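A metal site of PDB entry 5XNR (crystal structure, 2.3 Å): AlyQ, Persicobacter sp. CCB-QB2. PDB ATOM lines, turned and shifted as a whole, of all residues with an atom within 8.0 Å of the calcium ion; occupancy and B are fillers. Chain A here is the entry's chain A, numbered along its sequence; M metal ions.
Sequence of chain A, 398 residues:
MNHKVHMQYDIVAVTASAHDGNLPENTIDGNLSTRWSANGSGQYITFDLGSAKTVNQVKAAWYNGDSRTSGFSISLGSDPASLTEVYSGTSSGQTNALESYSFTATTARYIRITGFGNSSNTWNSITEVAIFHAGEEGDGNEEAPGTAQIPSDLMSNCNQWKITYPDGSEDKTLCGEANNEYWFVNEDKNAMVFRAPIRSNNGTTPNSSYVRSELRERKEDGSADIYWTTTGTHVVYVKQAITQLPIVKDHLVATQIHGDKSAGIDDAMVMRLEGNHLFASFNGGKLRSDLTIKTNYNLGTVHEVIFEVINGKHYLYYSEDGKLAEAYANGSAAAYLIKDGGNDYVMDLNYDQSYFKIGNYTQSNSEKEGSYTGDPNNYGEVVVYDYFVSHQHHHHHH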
ATOM      1  N   LEU A  23       6.416  17.492 -15.979  1.00  0.00           N
ATOM      2  CA  LEU A  23       7.113  18.457 -16.871  1.00  0.00           C
ATOM      3  C   LEU A  23       7.881  17.735 -17.981  1.00  0.00           C
ATOM      4  O   LEU A  23       8.250  16.572 -17.850  1.00  0.00           O
ATOM      5  CB  LEU A  23       8.040  19.335 -16.014  1.00  0.00           C
ATOM      6  CG  LEU A  23       7.347  20.158 -14.910  1.00  0.00           C
ATOM      7  CD1 LEU A  23       8.370  20.826 -13.992  1.00  0.00           C
ATOM      8  CD2 LEU A  23       6.436  21.216 -15.509  1.00  0.00           C
ATOM      9  N   PRO A  24       8.109  18.402 -19.094  1.00  0.00           N
ATOM     10  CA  PRO A  24       8.879  17.812 -20.204  1.00  0.00           C
ATOM     11  C   PRO A  24      10.301  17.350 -19.835  1.00  0.00           C
ATOM     12  O   PRO A  24      10.848  16.428 -20.473  1.00  0.00           O
ATOM     13  CB  PRO A  24       8.983  18.942 -21.257  1.00  0.00           C
ATOM     14  CG  PRO A  24       7.727  19.736 -21.051  1.00  0.00           C
ATOM     15  CD  PRO A  24       7.472  19.641 -19.555  1.00  0.00           C
ATOM     16  N   GLU A  25      10.890  17.987 -18.826  1.00  0.00           N
ATOM     17  CA  GLU A  25      12.270  17.720 -18.392  1.00  0.00           C
ATOM     18  C   GLU A  25      12.330  16.341 -17.734  1.00  0.00           C
ATOM     19  O   GLU A  25      13.385  15.735 -17.638  1.00  0.00           O
ATOM     20  CB  GLU A  25      12.740  18.775 -17.380  1.00  0.00           C
ATOM     21  CG  GLU A  25      13.031  20.132 -18.011  1.00  0.00           C
ATOM     22  CD  GLU A  25      11.811  20.953 -18.461  1.00  0.00           C
ATOM     23  OE1 GLU A  25      12.000  21.790 -19.373  1.00  0.00           O
ATOM     24  OE2 GLU A  25      10.684  20.756 -17.914  1.00  0.00           O
ATOM     25  N   ASN A  26      11.194  15.841 -17.297  1.00  0.00           N
ATOM     26  CA  ASN A  26      11.157  14.569 -16.640  1.00  0.00           C
ATOM     27  C   ASN A  26      11.629  13.498 -17.627  1.00  0.00           C
ATOM     28  O   ASN A  26      11.978  12.411 -17.189  1.00  0.00           O
ATOM     29  CB  ASN A  26       9.763  14.307 -16.044  1.00  0.00           C
ATOM     30  CG  ASN A  26       9.416  15.252 -14.899  1.00  0.00           C
ATOM     31  OD1 ASN A  26      10.298  15.956 -14.423  1.00  0.00           O
ATOM     32  ND2 ASN A  26       8.158  15.275 -14.466  1.00  0.00           N
ATOM     33  N   THR A  27      11.697  13.793 -18.938  1.00  0.00           N
ATOM     34  CA  THR A  27      12.028  12.749 -19.934  1.00  0.00           C
ATOM     35  C   THR A  27      13.541  12.535 -20.101  1.00  0.00           C
ATOM     36  O   THR A  27      13.946  11.621 -20.790  1.00  0.00           O
ATOM     37  CB  THR A  27      11.405  13.029 -21.301  1.00  0.00           C
ATOM     38  OG1 THR A  27      11.857  14.264 -21.870  1.00  0.00           O
ATOM     39  CG2 THR A  27       9.889  13.016 -21.221  1.00  0.00           C
ATOM     40  N   ILE A  28      14.380  13.365 -19.487  1.00  0.00           N
ATOM     41  CA  ILE A  28      15.811  13.262 -19.706  1.00  0.00           C
ATOM     42  C   ILE A  28      16.529  13.237 -18.358  1.00  0.00           C
ATOM     43  O   ILE A  28      17.680  13.608 -18.294  1.00  0.00           O
ATOM     44  CB  ILE A  28      16.296  14.425 -20.580  1.00  0.00           C
ATOM     45  CG1 ILE A  28      16.181  15.780 -19.870  1.00  0.00           C
ATOM     46  CG2 ILE A  28      15.551  14.445 -21.896  1.00  0.00           C
ATOM     47  CD1 ILE A  28      16.562  16.969 -20.735  1.00  0.00           C
ATOM     48  N   ASP A  29      15.865  12.800 -17.296  1.00  0.00           N
ATOM     49  CA  ASP A  29      16.476  12.858 -15.960  1.00  0.00           C
ATOM     50  C   ASP A  29      17.014  11.475 -15.582  1.00  0.00           C
ATOM     51  O   ASP A  29      17.558  11.303 -14.506  1.00  0.00           O
ATOM     52  CB  ASP A  29      15.514  13.449 -14.906  1.00  0.00           C
ATOM     53  CG  ASP A  29      14.195  12.717 -14.715  1.00  0.00           C
ATOM     54  OD1 ASP A  29      14.006  11.617 -15.318  1.00  0.00           O
ATOM     55  OD2 ASP A  29      13.346  13.258 -13.943  1.00  0.00           O
ATOM     56  N   GLY A  30      16.837  10.473 -16.447  1.00  0.00           N
ATOM     57  CA  GLY A  30      17.357   9.146 -16.140  1.00  0.00           C
ATOM     58  C   GLY A  30      16.511   8.425 -15.109  1.00  0.00           C
ATOM     59  O   GLY A  30      16.910   7.394 -14.596  1.00  0.00           O
ATOM     60  N   ASN A  31      15.317   8.940 -14.844  1.00  0.00           N
ATOM     61  CA  ASN A  31      14.495   8.477 -13.741  1.00  0.00           C
ATOM     62  C   ASN A  31      13.209   7.863 -14.315  1.00  0.00           C
ATOM     63  O   ASN A  31      12.446   8.550 -14.970  1.00  0.00           O
ATOM     64  CB  ASN A  31      14.211   9.636 -12.791  1.00  0.00           C
ATOM     65  CG  ASN A  31      13.570   9.197 -11.491  1.00  0.00           C
ATOM     66  OD1 ASN A  31      12.598   8.442 -11.486  1.00  0.00           O
ATOM     67  ND2 ASN A  31      14.130   9.676 -10.389  1.00  0.00           N
ATOM     68  N   LEU A  32      12.942   6.593 -14.031  1.00  0.00           N
ATOM     69  CA  LEU A  32      11.766   5.914 -14.606  1.00  0.00           C
ATOM     70  C   LEU A  32      10.470   6.306 -13.890  1.00  0.00           C
ATOM     71  O   LEU A  32       9.385   5.982 -14.371  1.00  0.00           O
ATOM     72  CB  LEU A  32      11.981   4.401 -14.519  1.00  0.00           C
ATOM     73  CG  LEU A  32      11.567   3.591 -15.756  1.00  0.00           C
ATOM     74  CD1 LEU A  32      11.891   4.329 -17.066  1.00  0.00           C
ATOM     75  CD2 LEU A  32      12.244   2.237 -15.729  1.00  0.00           C
ATOM     76  N   SER A  33      10.557   6.965 -12.730  1.00  0.00           N
ATOM     77  CA  SER A  33       9.347   7.230 -11.958  1.00  0.00           C
ATOM     78  C   SER A  33       8.890   8.685 -12.160  1.00  0.00           C
ATOM     79  O   SER A  33       7.907   9.030 -11.597  1.00  0.00           O
ATOM     80  CB  SER A  33       9.571   6.950 -10.497  1.00  0.00           C
ATOM     81  OG  SER A  33      10.489   7.879  -9.944  1.00  0.00           O
ATOM     82  N   THR A  34       9.627   9.508 -12.909  1.00  0.00           N
ATOM     83  CA  THR A  34       9.122  10.812 -13.344  1.00  0.00           C
ATOM     84  C   THR A  34       8.745  10.728 -14.822  1.00  0.00           C
ATOM     85  O   THR A  34       9.338   9.952 -15.578  1.00  0.00           O
ATOM     86  CB  THR A  34      10.151  11.931 -13.125  1.00  0.00           C
ATOM     87  OG1 THR A  34      11.309  11.621 -13.898  1.00  0.00           O
ATOM     88  CG2 THR A  34      10.554  12.099 -11.679  1.00  0.00           C
ATOM     89  N   ARG A  35       7.779  11.540 -15.250  1.00  0.00           N
ATOM     90  CA  ARG A  35       7.265  11.448 -16.622  1.00  0.00           C
ATOM     91  C   ARG A  35       6.817  12.822 -17.102  1.00  0.00           C
ATOM     92  O   ARG A  35       6.613  13.766 -16.309  1.00  0.00           O
ATOM     93  CB  ARG A  35       6.081  10.490 -16.661  1.00  0.00           C
ATOM     94  CG  ARG A  35       4.833  11.017 -15.952  1.00  0.00           C
ATOM     95  CD  ARG A  35       3.679  10.022 -15.945  1.00  0.00           C
ATOM     96  NE  ARG A  35       2.421  10.634 -15.526  1.00  0.00           N
ATOM     97  CZ  ARG A  35       1.912  10.554 -14.299  1.00  0.00           C
ATOM     98  NH1 ARG A  35       2.620  10.057 -13.297  1.00  0.00           N
ATOM     99  NH2 ARG A  35       0.663  10.956 -14.076  1.00  0.00           N
ATOM    100  N   TRP A  36       6.721  12.936 -18.425  1.00  0.00           N
ATOM    101  CA  TRP A  36       5.962  13.979 -19.076  1.00  0.00           C
ATOM    102  C   TRP A  36       4.555  13.434 -19.317  1.00  0.00           C
ATOM    103  O   TRP A  36       4.444  12.287 -19.670  1.00  0.00           O
ATOM    104  CB  TRP A  36       6.614  14.343 -20.404  1.00  0.00           C
ATOM    105  CG  TRP A  36       5.749  15.203 -21.277  1.00  0.00           C
ATOM    106  CD1 TRP A  36       5.320  16.455 -20.976  1.00  0.00           C
ATOM    107  CD2 TRP A  36       5.212  14.886 -22.577  1.00  0.00           C
ATOM    108  NE1 TRP A  36       4.535  16.935 -21.988  1.00  0.00           N
ATOM    109  CE2 TRP A  36       4.461  16.003 -22.990  1.00  0.00           C
ATOM    110  CE3 TRP A  36       5.278  13.765 -23.415  1.00  0.00           C
ATOM    111  CZ2 TRP A  36       3.794  16.043 -24.212  1.00  0.00           C
ATOM    112  CZ3 TRP A  36       4.609  13.801 -24.621  1.00  0.00           C
ATOM    113  CH2 TRP A  36       3.883  14.925 -25.013  1.00  0.00           C
ATOM    114  N   ALA A  61      10.944   5.516 -23.587  1.00  0.00           N
ATOM    115  CA  ALA A  61      10.330   4.563 -22.663  1.00  0.00           C
ATOM    116  C   ALA A  61       9.001   5.153 -22.177  1.00  0.00           C
ATOM    117  O   ALA A  61       8.923   6.333 -21.920  1.00  0.00           O
ATOM    118  CB  ALA A  61      11.268   4.270 -21.537  1.00  0.00           C
ATOM    119  N   ILE A 126       5.537   9.784 -21.227  1.00  0.00           N
ATOM    120  CA  ILE A 126       6.899   9.300 -21.562  1.00  0.00           C
ATOM    121  C   ILE A 126       7.787   9.456 -20.326  1.00  0.00           C
ATOM    122  O   ILE A 126       7.723  10.472 -19.666  1.00  0.00           O
ATOM    123  CB  ILE A 126       7.454  10.062 -22.789  1.00  0.00           C
ATOM    124  CG1 ILE A 126       6.545   9.852 -24.004  1.00  0.00           C
ATOM    125  CG2 ILE A 126       8.884   9.636 -23.070  1.00  0.00           C
ATOM    126  CD1 ILE A 126       6.862  10.718 -25.202  1.00  0.00           C
ATOM    127  N   THR A 127       8.536   8.416 -19.996  1.00  0.00           N
ATOM    128  CA  THR A 127       9.363   8.365 -18.782  1.00  0.00           C
ATOM    129  C   THR A 127      10.821   8.655 -19.129  1.00  0.00           C
ATOM    130  O   THR A 127      11.517   9.213 -18.338  1.00  0.00           O
ATOM    131  CB  THR A 127       9.272   7.004 -18.089  1.00  0.00           C
ATOM    132  OG1 THR A 127       9.631   5.977 -19.015  1.00  0.00           O
ATOM    133  CG2 THR A 127       7.900   6.686 -17.546  1.00  0.00           C
ATOM    134  N   GLU A 128      11.272   8.264 -20.318  1.00  0.00           N
ATOM    135  CA  GLU A 128      12.662   8.486 -20.739  1.00  0.00           C
ATOM    136  C   GLU A 128      12.725   8.579 -22.275  1.00  0.00           C
ATOM    137  O   GLU A 128      11.964   7.876 -22.973  1.00  0.00           O
ATOM    138  CB  GLU A 128      13.559   7.318 -20.350  1.00  0.00           C
ATOM    139  CG  GLU A 128      14.586   7.644 -19.291  1.00  0.00           C
ATOM    140  CD  GLU A 128      15.456   6.437 -18.966  1.00  0.00           C
ATOM    141  OE1 GLU A 128      16.172   5.960 -19.876  1.00  0.00           O
ATOM    142  OE2 GLU A 128      15.395   5.937 -17.814  1.00  0.00           O
ATOM    143  N   VAL A 129      13.641   9.415 -22.746  1.00  0.00           N
ATOM    144  CA  VAL A 129      13.919   9.576 -24.161  1.00  0.00           C
ATOM    145  C   VAL A 129      15.420   9.775 -24.365  1.00  0.00           C
ATOM    146  O   VAL A 129      16.074  10.496 -23.624  1.00  0.00           O
ATOM    147  CB  VAL A 129      13.113  10.750 -24.750  1.00  0.00           C
ATOM    148  CG1 VAL A 129      13.627  11.168 -26.112  1.00  0.00           C
ATOM    149  CG2 VAL A 129      11.643  10.409 -24.860  1.00  0.00           C
HETATM  150 CA    CA M   1      11.686  10.384 -16.206  1.00  0.00          CA
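ND2 of Asn 26 is in hydrogen-bond range of O of Arg 35 (2.8 Å). The side-chain amide nitrogen of Asn 26 sits close to the backbone NH of Leu 23, at 3.2 Å. The side-chain amide oxygen of Asn 31 is in hydrogen-bond range of the side-chain hydroxyl of Ser 33 (2.7 Å). The backbone carbonyl oxygen (O) of Ala 61 lies within hydrogen-bond range of the backbone NH (N) of Thr 127 (2.9 Å).
Five residues have an atom within 4 Å of the calcium ion: Asn 26, Asp 29, Asn 31, Thr 34 and Thr 127. The nearest printed residue that does not touch the calcium ion is Arg 35 (4.2 Å).
The calcium ion is bound by O of Asn 26, O of Asn 31, O of Thr 127, O of Thr 34, OG1 of Thr 34 and OD1 of Asp 29.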
